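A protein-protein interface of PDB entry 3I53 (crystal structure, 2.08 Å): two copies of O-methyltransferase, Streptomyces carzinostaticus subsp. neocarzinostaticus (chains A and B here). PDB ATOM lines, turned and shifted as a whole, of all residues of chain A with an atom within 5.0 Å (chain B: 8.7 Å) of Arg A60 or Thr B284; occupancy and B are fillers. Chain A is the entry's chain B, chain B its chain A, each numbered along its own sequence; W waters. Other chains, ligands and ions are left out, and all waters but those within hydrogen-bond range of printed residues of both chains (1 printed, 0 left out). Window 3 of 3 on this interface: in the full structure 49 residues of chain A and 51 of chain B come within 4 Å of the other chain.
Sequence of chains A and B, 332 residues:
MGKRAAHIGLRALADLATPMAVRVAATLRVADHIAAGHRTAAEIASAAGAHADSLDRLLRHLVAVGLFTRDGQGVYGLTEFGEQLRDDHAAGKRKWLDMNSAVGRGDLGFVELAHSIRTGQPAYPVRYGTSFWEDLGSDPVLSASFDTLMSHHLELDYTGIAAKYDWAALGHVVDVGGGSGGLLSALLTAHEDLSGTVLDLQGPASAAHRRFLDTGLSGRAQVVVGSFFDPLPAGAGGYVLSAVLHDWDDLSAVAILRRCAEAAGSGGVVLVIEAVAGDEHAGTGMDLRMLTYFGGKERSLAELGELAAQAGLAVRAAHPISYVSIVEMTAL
OG1 of Thr B284 sits at hydrogen-bond distance from ND1 of His A61, 2.9 Å away. The side-chain carboxylate (OD2) of Asp B287 lies within salt-bridge range of the guanidinium group (NE) of Arg A57.
OD1 of Asp B287 sits at hydrogen-bond distance from N of Glu B298 (3.2 Å). OD2 of Asp A56 is in salt-bridge range of NE of Arg A60, at 3.8 Å.
Among the printed residues, pairs that only touch across the chains: Arg A57 with Leu B291 (3.5 Å), Arg A60 with Thr B284 (3.6 Å), His A61 with Leu B288 (3.7 Å) and His A61 with Gly B285 (3.8 Å).
Of chain B, only Thr B284 comes within 4 Å of Arg A60. Of the printed residues of chain A, Thr B284 touches Arg A60 and His A61. Printed residues of chain B within 4 Å of Arg A57: Asp B287 (2.9 Å) and Leu B291 (3.5 Å). Of the printed residues of chain A, Leu B288 touches His A61 (3.7 Å). Of the printed residues of chain A, Asp B287 touches Arg A57 (2.9 Å). Of the printed residues of chain A, Gly B285 touches His A61 (3.8 Å). Printed residues of chain B within 4 Å of His A61: Thr B284 (2.9 Å), Gly B285 (3.8 Å) and Leu B288 (3.7 Å). Leu A58 touches none of the printed residues of chain B. The nearest residue of chain A that does not touch Thr B284 is Ala A64 (4.2 Å). The nearest printed residue of chain A that does not touch Asp B287 is Leu A58 (5.8 Å).
Of the 16 printed residues of chain B, 5 touch a printed residue of chain A. Hydrophobic or aromatic side chains of chain B within 4 Å of the printed part of chain A: Leu B288 and Leu B291. Of the 11 printed residues of chain A, 3 touch a printed residue of chain B. Hydrophobic or aromatic side chains of chain A within 4 Å of the printed part of chain B: His A61. Among the printed residues, Asp or Glu carboxylates within 4 Å of a Lys or Arg side-chain nitrogen of the other chain: Arg A57 with Asp B287.
No position is printed for both chains. Of the 6 pairs that touch across the chains among the printed residues, none has its exchanged pair printed and touching as well.
Water W1 lies within hydrogen-bond range of the backbone carbonyl oxygen of Arg A57 (2.7 Å) and the side-chain carboxylate of Asp B287 (2.7 Å).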
ATOM      1  N   ASP A  56       1.651 -17.713 -14.595  1.00  0.00           N
ATOM      2  CA  ASP A  56       1.337 -17.996 -13.204  1.00  0.00           C
ATOM      3  C   ASP A  56       1.534 -19.479 -12.889  1.00  0.00           C
ATOM      4  O   ASP A  56       1.957 -19.849 -11.790  1.00  0.00           O
ATOM      5  CB  ASP A  56      -0.102 -17.573 -12.903  1.00  0.00           C
ATOM      6  CG  ASP A  56      -0.500 -17.865 -11.478  1.00  0.00           C
ATOM      7  OD1 ASP A  56       0.279 -17.522 -10.563  1.00  0.00           O
ATOM      8  OD2 ASP A  56      -1.590 -18.437 -11.275  1.00  0.00           O
ATOM      9  N   ARG A  57       1.246 -20.330 -13.864  1.00  0.00           N
ATOM     10  CA  ARG A  57       1.405 -21.763 -13.666  1.00  0.00           C
ATOM     11  C   ARG A  57       2.884 -22.135 -13.597  1.00  0.00           C
ATOM     12  O   ARG A  57       3.278 -23.040 -12.855  1.00  0.00           O
ATOM     13  CB  ARG A  57       0.674 -22.519 -14.785  1.00  0.00           C
ATOM     14  CG  ARG A  57      -0.845 -22.391 -14.683  1.00  0.00           C
ATOM     15  CD  ARG A  57      -1.590 -22.871 -15.922  1.00  0.00           C
ATOM     16  NE  ARG A  57      -1.463 -24.305 -16.159  1.00  0.00           N
ATOM     17  CZ  ARG A  57      -2.062 -24.944 -17.162  1.00  0.00           C
ATOM     18  NH1 ARG A  57      -2.829 -24.274 -18.013  1.00  0.00           N
ATOM     19  NH2 ARG A  57      -1.885 -26.247 -17.329  1.00  0.00           N
ATOM     20  N   LEU A  58       3.710 -21.419 -14.355  1.00  0.00           N
ATOM     21  CA  LEU A  58       5.152 -21.668 -14.341  1.00  0.00           C
ATOM     22  C   LEU A  58       5.740 -21.227 -12.993  1.00  0.00           C
ATOM     23  O   LEU A  58       6.553 -21.931 -12.407  1.00  0.00           O
ATOM     24  CB  LEU A  58       5.861 -20.889 -15.461  1.00  0.00           C
ATOM     25  CG  LEU A  58       7.378 -21.115 -15.491  1.00  0.00           C
ATOM     26  CD1 LEU A  58       7.680 -22.465 -16.132  1.00  0.00           C
ATOM     27  CD2 LEU A  58       8.059 -20.006 -16.262  1.00  0.00           C
ATOM     28  N   LEU A  59       5.327 -20.050 -12.525  1.00  0.00           N
ATOM     29  CA  LEU A  59       5.813 -19.503 -11.262  1.00  0.00           C
ATOM     30  C   LEU A  59       5.430 -20.386 -10.082  1.00  0.00           C
ATOM     31  O   LEU A  59       6.219 -20.567  -9.155  1.00  0.00           O
ATOM     32  CB  LEU A  59       5.266 -18.085 -11.038  1.00  0.00           C
ATOM     33  CG  LEU A  59       5.772 -17.001 -11.991  1.00  0.00           C
ATOM     34  CD1 LEU A  59       5.341 -15.631 -11.489  1.00  0.00           C
ATOM     35  CD2 LEU A  59       7.283 -17.069 -12.077  1.00  0.00           C
ATOM     36  N   ARG A  60       4.215 -20.930 -10.118  1.00  0.00           N
ATOM     37  CA  ARG A  60       3.758 -21.791  -9.045  1.00  0.00           C
ATOM     38  C   ARG A  60       4.616 -23.042  -8.966  1.00  0.00           C
ATOM     39  O   ARG A  60       4.872 -23.573  -7.879  1.00  0.00           O
ATOM     40  CB  ARG A  60       2.294 -22.156  -9.253  1.00  0.00           C
ATOM     41  CG  ARG A  60       1.381 -20.970  -9.084  1.00  0.00           C
ATOM     42  CD  ARG A  60      -0.048 -21.400  -8.886  1.00  0.00           C
ATOM     43  NE  ARG A  60      -0.779 -20.399  -8.122  1.00  0.00           N
ATOM     44  CZ  ARG A  60      -1.671 -20.692  -7.183  1.00  0.00           C
ATOM     45  NH1 ARG A  60      -1.942 -21.960  -6.898  1.00  0.00           N
ATOM     46  NH2 ARG A  60      -2.284 -19.717  -6.523  1.00  0.00           N
ATOM     47  N   HIS A  61       5.067 -23.515 -10.123  1.00  0.00           N
ATOM     48  CA  HIS A  61       5.923 -24.686 -10.148  1.00  0.00           C
ATOM     49  C   HIS A  61       7.269 -24.306  -9.543  1.00  0.00           C
ATOM     50  O   HIS A  61       7.867 -25.084  -8.801  1.00  0.00           O
ATOM     51  CB  HIS A  61       6.143 -25.184 -11.578  1.00  0.00           C
ATOM     52  CG  HIS A  61       7.064 -26.358 -11.660  1.00  0.00           C
ATOM     53  ND1 HIS A  61       6.741 -27.593 -11.140  1.00  0.00           N
ATOM     54  CD2 HIS A  61       8.323 -26.474 -12.144  1.00  0.00           C
ATOM     55  CE1 HIS A  61       7.761 -28.418 -11.298  1.00  0.00           C
ATOM     56  NE2 HIS A  61       8.735 -27.763 -11.903  1.00  0.00           N
ATOM     57  N   LEU A  62       7.740 -23.103  -9.855  1.00  0.00           N
ATOM     58  CA  LEU A  62       9.026 -22.666  -9.338  1.00  0.00           C
ATOM     59  C   LEU A  62       8.984 -22.293  -7.856  1.00  0.00           C
ATOM     60  O   LEU A  62      10.013 -22.266  -7.183  1.00  0.00           O
ATOM     61  CB  LEU A  62       9.568 -21.521 -10.200  1.00  0.00           C
ATOM     62  CG  LEU A  62       9.715 -22.008 -11.648  1.00  0.00           C
ATOM     63  CD1 LEU A  62      10.249 -20.901 -12.561  1.00  0.00           C
ATOM     64  CD2 LEU A  62      10.632 -23.224 -11.665  1.00  0.00           C
ATOM     65  N   VAL A  63       7.788 -22.016  -7.352  1.00  0.00           N
ATOM     66  CA  VAL A  63       7.617 -21.709  -5.940  1.00  0.00           C
ATOM     67  C   VAL A  63       7.913 -23.023  -5.224  1.00  0.00           C
ATOM     68  O   VAL A  63       8.703 -23.072  -4.280  1.00  0.00           O
ATOM     69  CB  VAL A  63       6.162 -21.281  -5.632  1.00  0.00           C
ATOM     70  CG1 VAL A  63       5.906 -21.321  -4.133  1.00  0.00           C
ATOM     71  CG2 VAL A  63       5.910 -19.881  -6.166  1.00  0.00           C
ATOM     72  N   ALA A  64       7.291 -24.092  -5.714  1.00  0.00           N
ATOM     73  CA  ALA A  64       7.450 -25.429  -5.146  1.00  0.00           C
ATOM     74  C   ALA A  64       8.871 -25.950  -5.247  1.00  0.00           C
ATOM     75  O   ALA A  64       9.257 -26.851  -4.509  1.00  0.00           O
ATOM     76  CB  ALA A  64       6.504 -26.392  -5.832  1.00  0.00           C
ATOM     77  N   ARG A  70       5.451 -16.778  -2.885  1.00  0.00           N
ATOM     78  CA  ARG A  70       4.144 -16.296  -3.299  1.00  0.00           C
ATOM     79  C   ARG A  70       3.237 -16.166  -2.085  1.00  0.00           C
ATOM     80  O   ARG A  70       3.084 -17.125  -1.324  1.00  0.00           O
ATOM     81  CB  ARG A  70       3.530 -17.280  -4.298  1.00  0.00           C
ATOM     82  CG  ARG A  70       2.137 -16.914  -4.767  1.00  0.00           C
ATOM     83  CD  ARG A  70       1.550 -17.994  -5.667  1.00  0.00           C
ATOM     84  NE  ARG A  70       0.332 -17.550  -6.338  1.00  0.00           N
ATOM     85  CZ  ARG A  70      -0.842 -17.379  -5.740  1.00  0.00           C
ATOM     86  NH1 ARG A  70      -0.971 -17.620  -4.440  1.00  0.00           N
ATOM     87  NH2 ARG A  70      -1.890 -16.970  -6.444  1.00  0.00           N
ATOM     88  N   TYR A  76       4.326 -12.096  -5.831  1.00  0.00           N
ATOM     89  CA  TYR A  76       5.487 -12.975  -5.903  1.00  0.00           C
ATOM     90  C   TYR A  76       6.762 -12.305  -5.420  1.00  0.00           C
ATOM     91  O   TYR A  76       6.917 -11.096  -5.529  1.00  0.00           O
ATOM     92  CB  TYR A  76       5.712 -13.471  -7.341  1.00  0.00           C
ATOM     93  CG  TYR A  76       4.763 -14.561  -7.786  1.00  0.00           C
ATOM     94  CD1 TYR A  76       3.582 -14.256  -8.472  1.00  0.00           C
ATOM     95  CD2 TYR A  76       5.046 -15.900  -7.523  1.00  0.00           C
ATOM     96  CE1 TYR A  76       2.708 -15.261  -8.889  1.00  0.00           C
ATOM     97  CE2 TYR A  76       4.182 -16.914  -7.932  1.00  0.00           C
ATOM     98  CZ  TYR A  76       3.016 -16.590  -8.614  1.00  0.00           C
ATOM     99  OH  TYR A  76       2.165 -17.596  -9.017  1.00  0.00           O
ATOM    100  N   PHE B 110       8.743 -30.427 -23.804  1.00  0.00           N
ATOM    101  CA  PHE B 110       9.095 -29.448 -22.787  1.00  0.00           C
ATOM    102  C   PHE B 110      10.186 -28.525 -23.324  1.00  0.00           C
ATOM    103  O   PHE B 110      10.363 -27.402 -22.845  1.00  0.00           O
ATOM    104  CB  PHE B 110       9.587 -30.140 -21.510  1.00  0.00           C
ATOM    105  CG  PHE B 110       8.483 -30.506 -20.554  1.00  0.00           C
ATOM    106  CD1 PHE B 110       8.231 -31.833 -20.237  1.00  0.00           C
ATOM    107  CD2 PHE B 110       7.696 -29.519 -19.980  1.00  0.00           C
ATOM    108  CE1 PHE B 110       7.203 -32.179 -19.360  1.00  0.00           C
ATOM    109  CE2 PHE B 110       6.660 -29.846 -19.097  1.00  0.00           C
ATOM    110  CZ  PHE B 110       6.413 -31.175 -18.789  1.00  0.00           C
ATOM    111  N   ALA B 277      -6.638 -30.428  -7.967  1.00  0.00           N
ATOM    112  CA  ALA B 277      -5.482 -29.648  -7.544  1.00  0.00           C
ATOM    113  C   ALA B 277      -5.050 -29.958  -6.119  1.00  0.00           C
ATOM    114  O   ALA B 277      -3.946 -29.590  -5.712  1.00  0.00           O
ATOM    115  CB  ALA B 277      -5.772 -28.163  -7.687  1.00  0.00           C
ATOM    116  N   GLY B 278      -5.915 -30.632  -5.363  1.00  0.00           N
ATOM    117  CA  GLY B 278      -5.585 -30.983  -3.993  1.00  0.00           C
ATOM    118  C   GLY B 278      -4.607 -32.146  -3.900  1.00  0.00           C
ATOM    119  O   GLY B 278      -3.456 -32.051  -4.337  1.00  0.00           O
ATOM    120  N   ALA B 282      -1.519 -35.392  -8.850  1.00  0.00           N
ATOM    121  CA  ALA B 282      -0.240 -34.692  -8.919  1.00  0.00           C
ATOM    122  C   ALA B 282      -0.415 -33.184  -8.735  1.00  0.00           C
ATOM    123  O   ALA B 282      -1.523 -32.702  -8.476  1.00  0.00           O
ATOM    124  CB  ALA B 282       0.443 -34.981 -10.258  1.00  0.00           C
ATOM    125  N   GLY B 283       0.688 -32.450  -8.880  1.00  0.00           N
ATOM    126  CA  GLY B 283       0.662 -31.005  -8.720  1.00  0.00           C
ATOM    127  C   GLY B 283       1.220 -30.189  -9.878  1.00  0.00           C
ATOM    128  O   GLY B 283       0.924 -30.451 -11.049  1.00  0.00           O
ATOM    129  N   THR B 284       2.027 -29.186  -9.543  1.00  0.00           N
ATOM    130  CA  THR B 284       2.623 -28.292 -10.539  1.00  0.00           C
ATOM    131  C   THR B 284       3.314 -29.010 -11.696  1.00  0.00           C
ATOM    132  O   THR B 284       3.248 -28.545 -12.836  1.00  0.00           O
ATOM    133  CB  THR B 284       3.630 -27.322  -9.885  1.00  0.00           C
ATOM    134  OG1 THR B 284       4.654 -28.068  -9.211  1.00  0.00           O
ATOM    135  CG2 THR B 284       2.915 -26.403  -8.897  1.00  0.00           C
ATOM    136  N   GLY B 285       3.970 -30.133 -11.405  1.00  0.00           N
ATOM    137  CA  GLY B 285       4.653 -30.895 -12.442  1.00  0.00           C
ATOM    138  C   GLY B 285       3.735 -31.406 -13.549  1.00  0.00           C
ATOM    139  O   GLY B 285       3.997 -31.185 -14.736  1.00  0.00           O
ATOM    140  N   MET B 286       2.660 -32.091 -13.158  1.00  0.00           N
ATOM    141  CA  MET B 286       1.696 -32.634 -14.107  1.00  0.00           C
ATOM    142  C   MET B 286       0.974 -31.477 -14.791  1.00  0.00           C
ATOM    143  O   MET B 286       0.701 -31.522 -15.993  1.00  0.00           O
ATOM    144  CB  MET B 286       0.689 -33.539 -13.382  1.00  0.00           C
ATOM    145  CG  MET B 286      -0.201 -34.408 -14.312  1.00  0.00           C
ATOM    146  SD  MET B 286       0.704 -35.555 -15.470  1.00  0.00           S
ATOM    147  CE  MET B 286       1.336 -36.813 -14.337  1.00  0.00           C
ATOM    148  N   ASP B 287       0.673 -30.436 -14.022  1.00  0.00           N
ATOM    149  CA  ASP B 287       0.015 -29.264 -14.565  1.00  0.00           C
ATOM    150  C   ASP B 287       0.779 -28.763 -15.799  1.00  0.00           C
ATOM    151  O   ASP B 287       0.186 -28.511 -16.852  1.00  0.00           O
ATOM    152  CB  ASP B 287      -0.036 -28.145 -13.534  1.00  0.00           C
ATOM    153  CG  ASP B 287      -0.698 -26.895 -14.075  1.00  0.00           C
ATOM    154  OD1 ASP B 287      -1.890 -26.966 -14.443  1.00  0.00           O
ATOM    155  OD2 ASP B 287      -0.027 -25.847 -14.147  1.00  0.00           O
ATOM    156  N   LEU B 288       2.091 -28.606 -15.657  1.00  0.00           N
ATOM    157  CA  LEU B 288       2.907 -28.149 -16.768  1.00  0.00           C
ATOM    158  C   LEU B 288       2.901 -29.165 -17.915  1.00  0.00           C
ATOM    159  O   LEU B 288       2.910 -28.771 -19.085  1.00  0.00           O
ATOM    160  CB  LEU B 288       4.338 -27.868 -16.308  1.00  0.00           C
ATOM    161  CG  LEU B 288       4.531 -26.626 -15.421  1.00  0.00           C
ATOM    162  CD1 LEU B 288       6.013 -26.396 -15.169  1.00  0.00           C
ATOM    163  CD2 LEU B 288       3.917 -25.401 -16.093  1.00  0.00           C
ATOM    164  N   ARG B 289       2.883 -30.460 -17.583  1.00  0.00           N
ATOM    165  CA  ARG B 289       2.854 -31.494 -18.610  1.00  0.00           C
ATOM    166  C   ARG B 289       1.571 -31.340 -19.423  1.00  0.00           C
ATOM    167  O   ARG B 289       1.591 -31.405 -20.654  1.00  0.00           O
ATOM    168  CB  ARG B 289       2.913 -32.908 -17.996  1.00  0.00           C
ATOM    169  CG  ARG B 289       2.846 -34.023 -19.075  1.00  0.00           C
ATOM    170  CD  ARG B 289       3.130 -35.452 -18.570  1.00  0.00           C
ATOM    171  NE  ARG B 289       4.551 -35.723 -18.347  1.00  0.00           N
ATOM    172  CZ  ARG B 289       5.199 -35.456 -17.215  1.00  0.00           C
ATOM    173  NH1 ARG B 289       4.557 -34.905 -16.184  1.00  0.00           N
ATOM    174  NH2 ARG B 289       6.490 -35.745 -17.101  1.00  0.00           N
ATOM    175  N   MET B 290       0.455 -31.130 -18.727  1.00  0.00           N
ATOM    176  CA  MET B 290      -0.834 -30.953 -19.387  1.00  0.00           C
ATOM    177  C   MET B 290      -0.774 -29.723 -20.301  1.00  0.00           C
ATOM    178  O   MET B 290      -1.260 -29.753 -21.428  1.00  0.00           O
ATOM    179  CB  MET B 290      -1.944 -30.789 -18.350  1.00  0.00           C
ATOM    180  CG  MET B 290      -2.221 -32.046 -17.546  1.00  0.00           C
ATOM    181  SD  MET B 290      -2.804 -33.420 -18.582  1.00  0.00           S
ATOM    182  CE  MET B 290      -1.237 -34.309 -18.913  1.00  0.00           C
ATOM    183  N   LEU B 291      -0.180 -28.642 -19.806  1.00  0.00           N
ATOM    184  CA  LEU B 291      -0.042 -27.437 -20.607  1.00  0.00           C
ATOM    185  C   LEU B 291       0.812 -27.674 -21.867  1.00  0.00           C
ATOM    186  O   LEU B 291       0.426 -27.275 -22.966  1.00  0.00           O
ATOM    187  CB  LEU B 291       0.583 -26.307 -19.781  1.00  0.00           C
ATOM    188  CG  LEU B 291       0.979 -25.058 -20.571  1.00  0.00           C
ATOM    189  CD1 LEU B 291      -0.250 -24.412 -21.258  1.00  0.00           C
ATOM    190  CD2 LEU B 291       1.652 -24.091 -19.619  1.00  0.00           C
ATOM    191  N   GLU B 298      -4.410 -28.951 -14.732  1.00  0.00           N
ATOM    192  CA  GLU B 298      -4.912 -29.612 -13.540  1.00  0.00           C
ATOM    193  C   GLU B 298      -5.817 -28.573 -12.902  1.00  0.00           C
ATOM    194  O   GLU B 298      -5.474 -27.387 -12.852  1.00  0.00           O
ATOM    195  CB  GLU B 298      -3.786 -29.965 -12.573  1.00  0.00           C
ATOM    196  CG  GLU B 298      -3.038 -31.250 -12.907  1.00  0.00           C
ATOM    197  CD  GLU B 298      -2.328 -31.828 -11.691  1.00  0.00           C
ATOM    198  OE1 GLU B 298      -1.545 -31.085 -11.047  1.00  0.00           O
ATOM    199  OE2 GLU B 298      -2.556 -33.024 -11.378  1.00  0.00           O
ATOM    200  N   SER B 300      -8.676 -27.426  -9.630  1.00  0.00           N
ATOM    201  CA  SER B 300      -9.091 -27.633  -8.248  1.00  0.00           C
ATOM    202  C   SER B 300     -10.573 -28.006  -8.293  1.00  0.00           C
ATOM    203  O   SER B 300     -11.215 -27.898  -9.332  1.00  0.00           O
ATOM    204  CB  SER B 300      -8.950 -26.345  -7.462  1.00  0.00           C
ATOM    205  OG  SER B 300      -9.919 -25.423  -7.924  1.00  0.00           O
ATOM    206  N   GLU B 303     -12.369 -24.924  -9.421  1.00  0.00           N
ATOM    207  CA  GLU B 303     -12.305 -24.628 -10.853  1.00  0.00           C
ATOM    208  C   GLU B 303     -13.233 -25.595 -11.575  1.00  0.00           C
ATOM    209  O   GLU B 303     -13.872 -25.244 -12.567  1.00  0.00           O
ATOM    210  CB  GLU B 303     -10.851 -24.744 -11.350  1.00  0.00           C
ATOM    211  CG  GLU B 303      -9.942 -23.693 -10.679  1.00  0.00           C
ATOM    212  CD  GLU B 303      -8.459 -23.882 -10.947  1.00  0.00           C
ATOM    213  OE1 GLU B 303      -7.955 -25.012 -10.773  1.00  0.00           O
ATOM    214  OE2 GLU B 303      -7.789 -22.887 -11.314  1.00  0.00           O
HETATM  215  O   HOH W   1       1.409 -24.842 -12.068  1.00  0.00           O
